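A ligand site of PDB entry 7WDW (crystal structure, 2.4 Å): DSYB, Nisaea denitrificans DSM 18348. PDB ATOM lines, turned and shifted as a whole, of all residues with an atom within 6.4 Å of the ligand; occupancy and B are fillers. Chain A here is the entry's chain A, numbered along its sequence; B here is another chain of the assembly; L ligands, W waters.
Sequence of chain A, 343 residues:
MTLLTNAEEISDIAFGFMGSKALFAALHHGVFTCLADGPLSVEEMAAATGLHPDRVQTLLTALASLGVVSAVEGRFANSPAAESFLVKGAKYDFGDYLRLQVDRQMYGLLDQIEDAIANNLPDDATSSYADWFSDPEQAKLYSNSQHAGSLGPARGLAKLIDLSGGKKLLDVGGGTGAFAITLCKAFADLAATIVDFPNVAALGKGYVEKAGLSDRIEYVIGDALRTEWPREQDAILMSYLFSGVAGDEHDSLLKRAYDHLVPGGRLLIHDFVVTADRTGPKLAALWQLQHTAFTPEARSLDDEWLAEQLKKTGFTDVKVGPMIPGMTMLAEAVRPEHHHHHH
The side-chain hydroxyl (OG) of Ser 150 lies within hydrogen-bond range of the backbone carbonyl oxygen (O) of Gln 146 (3.2 Å). The backbone NH of Met 106 sits at hydrogen-bond distance from the backbone carbonyl oxygen of Gln 101, 3.1 Å away. O of His 270 sits at hydrogen-bond distance from N of Tyr 240 (2.7 Å). O of Tyr 142 is in hydrogen-bond range of NE2 of Gln 101 (3.3 Å). The side-chain amide nitrogen (NE2) of Gln 101 sits close to the backbone NH (N) of Gln 146 (3.4 Å). OH of Tyr 142 sits at hydrogen-bond distance from OH of Tyr 129, 2.9 Å away.
Water W1 lies within hydrogen-bond range of the side-chain hydroxyl of Tyr 240, an oxygen (O3) of the ligand and the side-chain hydroxyl of Ser 150.
S1 of the ligand lies close to OE1 of Gln 146 (3.2 Å). OH of Tyr 240 lies within hydrogen-bond range of O1 of the ligand (2.8 Å). OE1 of Gln 101 sits close to S1 of the ligand, at 3.1 Å.
O of Gly 149 sits close to O3 of the ligand (3.3 Å). Tyr 97 touches the ligand (OH to C4, 3.3 Å). Tyr 142 touches the ligand (OH to C1, 3.0 Å). Ser 150 touches the ligand (N to O3, 3.7 Å). Trp 287 touches the ligand. NE2 of His 291 touches C1 of the ligand (2.8 Å). Within 4 Å of the ligand: Tyr 97, Gln 101, Tyr 142, Gln 146, Gly 149, Ser 150, Tyr 240, Trp 287 and His 291. The nearest printed residue that does not touch the ligand is Phe 272 (4.02 Å).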
ATOM      1  N   TYR A  97       4.967   0.282  18.216  1.00  0.00           N
ATOM      2  CA  TYR A  97       5.082  -1.163  18.467  1.00  0.00           C
ATOM      3  C   TYR A  97       4.601  -1.470  19.885  1.00  0.00           C
ATOM      4  O   TYR A  97       3.963  -2.490  20.139  1.00  0.00           O
ATOM      5  CB  TYR A  97       6.525  -1.645  18.253  1.00  0.00           C
ATOM      6  CG  TYR A  97       6.849  -2.967  18.919  1.00  0.00           C
ATOM      7  CD1 TYR A  97       6.457  -4.182  18.363  1.00  0.00           C
ATOM      8  CD2 TYR A  97       7.580  -3.006  20.099  1.00  0.00           C
ATOM      9  CE1 TYR A  97       6.754  -5.379  18.967  1.00  0.00           C
ATOM     10  CE2 TYR A  97       7.879  -4.199  20.712  1.00  0.00           C
ATOM     11  CZ  TYR A  97       7.465  -5.386  20.146  1.00  0.00           C
ATOM     12  OH  TYR A  97       7.775  -6.562  20.773  1.00  0.00           O
ATOM     13  N   GLN A 101       0.979  -3.481  19.365  1.00  0.00           N
ATOM     14  CA  GLN A 101       1.208  -4.910  19.563  1.00  0.00           C
ATOM     15  C   GLN A 101       1.348  -5.340  21.037  1.00  0.00           C
ATOM     16  O   GLN A 101       0.660  -6.262  21.475  1.00  0.00           O
ATOM     17  CB  GLN A 101       2.388  -5.436  18.741  1.00  0.00           C
ATOM     18  CG  GLN A 101       2.487  -6.963  18.777  1.00  0.00           C
ATOM     19  CD  GLN A 101       3.824  -7.503  18.261  1.00  0.00           C
ATOM     20  OE1 GLN A 101       4.485  -8.279  18.947  1.00  0.00           O
ATOM     21  NE2 GLN A 101       4.198  -7.112  17.050  1.00  0.00           N
ATOM     22  N   MET A 106      -0.736  -8.161  23.471  1.00  0.00           N
ATOM     23  CA  MET A 106      -0.012  -9.087  24.357  1.00  0.00           C
ATOM     24  C   MET A 106      -0.486  -9.075  25.811  1.00  0.00           C
ATOM     25  O   MET A 106      -0.693 -10.136  26.406  1.00  0.00           O
ATOM     26  CB  MET A 106       1.482  -8.827  24.298  1.00  0.00           C
ATOM     27  CG  MET A 106       2.099  -9.125  22.950  1.00  0.00           C
ATOM     28  SD  MET A 106       2.054 -10.893  22.538  1.00  0.00           S
ATOM     29  CE  MET A 106       2.645 -10.840  20.867  1.00  0.00           C
ATOM     30  N   TYR A 129      -0.820 -19.179  16.483  1.00  0.00           N
ATOM     31  CA  TYR A 129      -0.697 -18.109  15.511  1.00  0.00           C
ATOM     32  C   TYR A 129      -1.753 -18.237  14.409  1.00  0.00           C
ATOM     33  O   TYR A 129      -2.371 -17.258  13.992  1.00  0.00           O
ATOM     34  CB  TYR A 129       0.691 -18.156  14.896  1.00  0.00           C
ATOM     35  CG  TYR A 129       1.714 -17.240  15.528  1.00  0.00           C
ATOM     36  CD1 TYR A 129       1.505 -15.865  15.582  1.00  0.00           C
ATOM     37  CD2 TYR A 129       2.916 -17.741  16.009  1.00  0.00           C
ATOM     38  CE1 TYR A 129       2.457 -15.024  16.124  1.00  0.00           C
ATOM     39  CE2 TYR A 129       3.867 -16.916  16.537  1.00  0.00           C
ATOM     40  CZ  TYR A 129       3.639 -15.569  16.605  1.00  0.00           C
ATOM     41  OH  TYR A 129       4.600 -14.763  17.139  1.00  0.00           O
ATOM     42  N   TYR A 142      -0.986  -7.220  14.301  1.00  0.00           N
ATOM     43  CA  TYR A 142       0.249  -7.804  14.813  1.00  0.00           C
ATOM     44  C   TYR A 142       1.405  -7.591  13.839  1.00  0.00           C
ATOM     45  O   TYR A 142       2.500  -7.154  14.232  1.00  0.00           O
ATOM     46  CB  TYR A 142       0.045  -9.301  15.102  1.00  0.00           C
ATOM     47  CG  TYR A 142       1.301 -10.006  15.533  1.00  0.00           C
ATOM     48  CD1 TYR A 142       2.197 -10.518  14.597  1.00  0.00           C
ATOM     49  CD2 TYR A 142       1.618 -10.147  16.873  1.00  0.00           C
ATOM     50  CE1 TYR A 142       3.338 -11.153  15.000  1.00  0.00           C
ATOM     51  CE2 TYR A 142       2.760 -10.782  17.276  1.00  0.00           C
ATOM     52  CZ  TYR A 142       3.625 -11.285  16.339  1.00  0.00           C
ATOM     53  OH  TYR A 142       4.767 -11.920  16.742  1.00  0.00           O
ATOM     54  N   SER A 145       3.112  -3.880  13.245  1.00  0.00           N
ATOM     55  CA  SER A 145       4.059  -3.455  14.264  1.00  0.00           C
ATOM     56  C   SER A 145       5.262  -4.399  14.345  1.00  0.00           C
ATOM     57  O   SER A 145       6.395  -3.962  14.635  1.00  0.00           O
ATOM     58  CB  SER A 145       3.383  -3.359  15.629  1.00  0.00           C
ATOM     59  OG  SER A 145       2.430  -2.314  15.629  1.00  0.00           O
ATOM     60  N   GLN A 146       5.018  -5.687  14.109  1.00  0.00           N
ATOM     61  CA  GLN A 146       6.078  -6.686  14.077  1.00  0.00           C
ATOM     62  C   GLN A 146       7.103  -6.301  13.011  1.00  0.00           C
ATOM     63  O   GLN A 146       8.319  -6.337  13.255  1.00  0.00           O
ATOM     64  CB  GLN A 146       5.493  -8.065  13.768  1.00  0.00           C
ATOM     65  CG  GLN A 146       6.540  -9.171  13.641  1.00  0.00           C
ATOM     66  CD  GLN A 146       7.294  -9.368  14.931  1.00  0.00           C
ATOM     67  OE1 GLN A 146       6.805  -9.001  15.992  1.00  0.00           O
ATOM     68  NE2 GLN A 146       8.490  -9.927  14.845  1.00  0.00           N
ATOM     69  N   HIS A 147       6.583  -5.960  11.828  1.00  0.00           N
ATOM     70  CA  HIS A 147       7.378  -5.500  10.680  1.00  0.00           C
ATOM     71  C   HIS A 147       8.245  -4.328  11.088  1.00  0.00           C
ATOM     72  O   HIS A 147       9.473  -4.376  10.997  1.00  0.00           O
ATOM     73  CB  HIS A 147       6.432  -5.068   9.552  1.00  0.00           C
ATOM     74  CG  HIS A 147       7.059  -5.088   8.193  1.00  0.00           C
ATOM     75  ND1 HIS A 147       8.002  -4.161   7.789  1.00  0.00           N
ATOM     76  CD2 HIS A 147       6.872  -5.918   7.138  1.00  0.00           C
ATOM     77  CE1 HIS A 147       8.359  -4.417   6.542  1.00  0.00           C
ATOM     78  NE2 HIS A 147       7.692  -5.475   6.126  1.00  0.00           N
ATOM     79  N   ALA A 148       7.576  -3.257  11.526  1.00  0.00           N
ATOM     80  CA  ALA A 148       8.231  -2.063  12.005  1.00  0.00           C
ATOM     81  C   ALA A 148       9.350  -2.377  12.984  1.00  0.00           C
ATOM     82  O   ALA A 148      10.442  -1.780  12.914  1.00  0.00           O
ATOM     83  CB  ALA A 148       7.220  -1.112  12.633  1.00  0.00           C
ATOM     84  N   GLY A 149       9.099  -3.330  13.887  1.00  0.00           N
ATOM     85  CA  GLY A 149      10.045  -3.681  14.925  1.00  0.00           C
ATOM     86  C   GLY A 149      11.248  -4.492  14.477  1.00  0.00           C
ATOM     87  O   GLY A 149      12.298  -4.458  15.105  1.00  0.00           O
ATOM     88  N   SER A 150      11.094  -5.207  13.358  1.00  0.00           N
ATOM     89  CA  SER A 150      12.127  -6.111  12.838  1.00  0.00           C
ATOM     90  C   SER A 150      13.116  -5.441  11.882  1.00  0.00           C
ATOM     91  O   SER A 150      14.203  -5.963  11.640  1.00  0.00           O
ATOM     92  CB  SER A 150      11.468  -7.297  12.147  1.00  0.00           C
ATOM     93  OG  SER A 150      10.920  -8.205  13.088  1.00  0.00           O
ATOM     94  N   LEU A 151      12.733  -4.281  11.326  1.00  0.00           N
ATOM     95  CA  LEU A 151      13.592  -3.582  10.373  1.00  0.00           C
ATOM     96  C   LEU A 151      14.976  -3.292  10.928  1.00  0.00           C
ATOM     97  O   LEU A 151      15.975  -3.521  10.262  1.00  0.00           O
ATOM     98  CB  LEU A 151      12.957  -2.272   9.892  1.00  0.00           C
ATOM     99  CG  LEU A 151      11.778  -2.353   8.937  1.00  0.00           C
ATOM    100  CD1 LEU A 151      11.280  -0.945   8.594  1.00  0.00           C
ATOM    101  CD2 LEU A 151      12.142  -3.124   7.682  1.00  0.00           C
ATOM    102  N   PRO A 153      16.660  -4.790  13.505  1.00  0.00           N
ATOM    103  CA  PRO A 153      17.411  -6.040  13.684  1.00  0.00           C
ATOM    104  C   PRO A 153      17.867  -6.633  12.352  1.00  0.00           C
ATOM    105  O   PRO A 153      18.922  -7.285  12.268  1.00  0.00           O
ATOM    106  CB  PRO A 153      16.398  -6.968  14.348  1.00  0.00           C
ATOM    107  CG  PRO A 153      15.380  -6.048  15.002  1.00  0.00           C
ATOM    108  CD  PRO A 153      15.311  -4.846  14.105  1.00  0.00           C
ATOM    109  N   TYR A 240      11.909 -15.841  15.184  1.00  0.00           N
ATOM    110  CA  TYR A 240      10.743 -15.995  16.069  1.00  0.00           C
ATOM    111  C   TYR A 240       9.816 -17.096  15.581  1.00  0.00           C
ATOM    112  O   TYR A 240       8.608 -17.012  15.754  1.00  0.00           O
ATOM    113  CB  TYR A 240       9.935 -14.702  16.174  1.00  0.00           C
ATOM    114  CG  TYR A 240      10.724 -13.494  16.598  1.00  0.00           C
ATOM    115  CD1 TYR A 240      11.295 -13.415  17.867  1.00  0.00           C
ATOM    116  CD2 TYR A 240      10.880 -12.417  15.740  1.00  0.00           C
ATOM    117  CE1 TYR A 240      12.009 -12.302  18.254  1.00  0.00           C
ATOM    118  CE2 TYR A 240      11.594 -11.295  16.123  1.00  0.00           C
ATOM    119  CZ  TYR A 240      12.152 -11.246  17.374  1.00  0.00           C
ATOM    120  OH  TYR A 240      12.873 -10.136  17.728  1.00  0.00           O
ATOM    121  N   HIS A 270      16.857 -16.710  14.734  1.00  0.00           N
ATOM    122  CA  HIS A 270      16.791 -15.549  15.598  1.00  0.00           C
ATOM    123  C   HIS A 270      15.589 -15.687  16.523  1.00  0.00           C
ATOM    124  O   HIS A 270      14.451 -15.892  16.090  1.00  0.00           O
ATOM    125  CB  HIS A 270      16.668 -14.291  14.760  1.00  0.00           C
ATOM    126  CG  HIS A 270      16.546 -13.045  15.572  1.00  0.00           C
ATOM    127  ND1 HIS A 270      15.504 -12.151  15.407  1.00  0.00           N
ATOM    128  CD2 HIS A 270      17.327 -12.535  16.552  1.00  0.00           C
ATOM    129  CE1 HIS A 270      15.656 -11.152  16.249  1.00  0.00           C
ATOM    130  NE2 HIS A 270      16.754 -11.356  16.953  1.00  0.00           N
ATOM    131  N   PHE A 272      14.170 -15.540  21.090  1.00  0.00           N
ATOM    132  CA  PHE A 272      14.378 -15.502  22.529  1.00  0.00           C
ATOM    133  C   PHE A 272      15.104 -16.768  22.926  1.00  0.00           C
ATOM    134  O   PHE A 272      14.587 -17.865  22.761  1.00  0.00           O
ATOM    135  CB  PHE A 272      13.033 -15.417  23.254  1.00  0.00           C
ATOM    136  CG  PHE A 272      12.137 -14.355  22.702  1.00  0.00           C
ATOM    137  CD1 PHE A 272      12.479 -13.013  22.826  1.00  0.00           C
ATOM    138  CD2 PHE A 272      10.996 -14.688  21.995  1.00  0.00           C
ATOM    139  CE1 PHE A 272      11.695 -12.028  22.284  1.00  0.00           C
ATOM    140  CE2 PHE A 272      10.181 -13.699  21.444  1.00  0.00           C
ATOM    141  CZ  PHE A 272      10.536 -12.367  21.592  1.00  0.00           C
ATOM    142  N   TRP A 287       9.701 -13.246  27.411  1.00  0.00           N
ATOM    143  CA  TRP A 287       9.065 -13.323  26.105  1.00  0.00           C
ATOM    144  C   TRP A 287       8.768 -14.769  25.682  1.00  0.00           C
ATOM    145  O   TRP A 287       7.814 -15.013  24.936  1.00  0.00           O
ATOM    146  CB  TRP A 287       9.911 -12.614  25.051  1.00  0.00           C
ATOM    147  CG  TRP A 287       9.450 -11.213  24.761  1.00  0.00           C
ATOM    148  CD1 TRP A 287      10.020 -10.052  25.199  1.00  0.00           C
ATOM    149  CD2 TRP A 287       8.312 -10.833  23.964  1.00  0.00           C
ATOM    150  NE1 TRP A 287       9.303  -8.973  24.718  1.00  0.00           N
ATOM    151  CE2 TRP A 287       8.267  -9.421  23.961  1.00  0.00           C
ATOM    152  CE3 TRP A 287       7.341 -11.549  23.260  1.00  0.00           C
ATOM    153  CZ2 TRP A 287       7.274  -8.723  23.282  1.00  0.00           C
ATOM    154  CZ3 TRP A 287       6.358 -10.851  22.581  1.00  0.00           C
ATOM    155  CH2 TRP A 287       6.327  -9.446  22.611  1.00  0.00           C
ATOM    156  N   HIS A 291       4.986 -15.897  24.623  1.00  0.00           N
ATOM    157  CA  HIS A 291       4.615 -16.705  23.461  1.00  0.00           C
ATOM    158  C   HIS A 291       3.854 -17.953  23.883  1.00  0.00           C
ATOM    159  O   HIS A 291       2.926 -18.388  23.195  1.00  0.00           O
ATOM    160  CB  HIS A 291       5.833 -17.037  22.605  1.00  0.00           C
ATOM    161  CG  HIS A 291       6.177 -15.947  21.632  1.00  0.00           C
ATOM    162  ND1 HIS A 291       6.321 -16.168  20.285  1.00  0.00           N
ATOM    163  CD2 HIS A 291       6.344 -14.620  21.815  1.00  0.00           C
ATOM    164  CE1 HIS A 291       6.587 -15.035  19.675  1.00  0.00           C
ATOM    165  NE2 HIS A 291       6.594 -14.073  20.573  1.00  0.00           N
ATOM    166  N   PHE A 294      -0.078 -18.196  23.840  1.00  0.00           N
ATOM    167  CA  PHE A 294      -0.854 -18.505  22.641  1.00  0.00           C
ATOM    168  C   PHE A 294      -0.177 -19.614  21.835  1.00  0.00           C
ATOM    169  O   PHE A 294      -0.409 -19.781  20.630  1.00  0.00           O
ATOM    170  CB  PHE A 294      -1.100 -17.249  21.786  1.00  0.00           C
ATOM    171  CG  PHE A 294       0.154 -16.531  21.370  1.00  0.00           C
ATOM    172  CD1 PHE A 294       0.889 -16.970  20.267  1.00  0.00           C
ATOM    173  CD2 PHE A 294       0.613 -15.425  22.075  1.00  0.00           C
ATOM    174  CE1 PHE A 294       2.066 -16.325  19.892  1.00  0.00           C
ATOM    175  CE2 PHE A 294       1.789 -14.771  21.696  1.00  0.00           C
ATOM    176  CZ  PHE A 294       2.515 -15.218  20.598  1.00  0.00           C
ATOM    177  N   ILE A 324      19.319  -8.670  19.596  1.00  0.00           N
ATOM    178  CA  ILE A 324      18.651  -7.601  20.309  1.00  0.00           C
ATOM    179  C   ILE A 324      19.072  -7.710  21.764  1.00  0.00           C
ATOM    180  O   ILE A 324      18.725  -8.663  22.448  1.00  0.00           O
ATOM    181  CB  ILE A 324      17.133  -7.679  20.161  1.00  0.00           C
ATOM    182  CG1 ILE A 324      16.742  -7.418  18.701  1.00  0.00           C
ATOM    183  CG2 ILE A 324      16.458  -6.667  21.073  1.00  0.00           C
ATOM    184  CD1 ILE A 324      15.349  -7.911  18.335  1.00  0.00           C
ATOM    185  N   MET A 327      17.634  -9.451  24.947  1.00  0.00           N
ATOM    186  CA  MET A 327      16.358  -9.988  24.465  1.00  0.00           C
ATOM    187  C   MET A 327      16.446 -11.209  23.537  1.00  0.00           C
ATOM    188  O   MET A 327      15.892 -12.250  23.834  1.00  0.00           O
ATOM    189  CB  MET A 327      15.548  -8.889  23.788  1.00  0.00           C
ATOM    190  CG  MET A 327      14.097  -9.293  23.533  1.00  0.00           C
ATOM    191  SD  MET A 327      13.021  -7.877  23.320  1.00  0.00           S
ATOM    192  CE  MET A 327      13.840  -6.743  24.431  1.00  0.00           C
ATOM    193  N   THR A 328      17.119 -11.076  22.402  1.00  0.00           N
ATOM    194  CA  THR A 328      17.207 -12.180  21.466  1.00  0.00           C
ATOM    195  C   THR A 328      18.649 -12.612  21.242  1.00  0.00           C
ATOM    196  O   THR A 328      19.591 -11.909  21.615  1.00  0.00           O
ATOM    197  CB  THR A 328      16.625 -11.827  20.089  1.00  0.00           C
ATOM    198  OG1 THR A 328      17.274 -10.667  19.575  1.00  0.00           O
ATOM    199  CG2 THR A 328      15.155 -11.588  20.170  1.00  0.00           C
ATOM    200  N   PHE B  15       7.913  -4.564  29.396  1.00  0.00           N
ATOM    201  CA  PHE B  15       7.636  -5.982  29.572  1.00  0.00           C
ATOM    202  C   PHE B  15       7.613  -6.417  31.024  1.00  0.00           C
ATOM    203  O   PHE B  15       7.565  -7.622  31.343  1.00  0.00           O
ATOM    204  CB  PHE B  15       8.659  -6.795  28.783  1.00  0.00           C
ATOM    205  CG  PHE B  15       8.816  -6.353  27.356  1.00  0.00           C
ATOM    206  CD1 PHE B  15       7.708  -6.100  26.567  1.00  0.00           C
ATOM    207  CD2 PHE B  15      10.070  -6.187  26.796  1.00  0.00           C
ATOM    208  CE1 PHE B  15       7.845  -5.699  25.225  1.00  0.00           C
ATOM    209  CE2 PHE B  15      10.220  -5.787  25.476  1.00  0.00           C
ATOM    210  CZ  PHE B  15       9.101  -5.538  24.678  1.00  0.00           C
HETATM  211  C1  LIG L   1       6.665 -11.648  19.108  1.00  0.00           C
HETATM  212  S1  LIG L   1       7.083  -9.896  19.011  1.00  0.00           S
HETATM  213  C2  LIG L   1       8.886  -9.691  19.093  1.00  0.00           C
HETATM  214  C3  LIG L   1       9.341  -8.602  18.128  1.00  0.00           C
HETATM  215  C4  LIG L   1      10.239  -7.628  18.883  1.00  0.00           C
HETATM  216  C5  LIG L   1      10.593  -6.435  17.995  1.00  0.00           C
HETATM  217  O1  LIG L   1      11.419  -8.268  19.272  1.00  0.00           O
HETATM  218  O2  LIG L   1      11.227  -5.470  18.477  1.00  0.00           O
HETATM  219  O3  LIG L   1      10.260  -6.426  16.780  1.00  0.00           O
HETATM  220  O   HOH W   1      12.272  -8.166  15.959  1.00  0.00           O
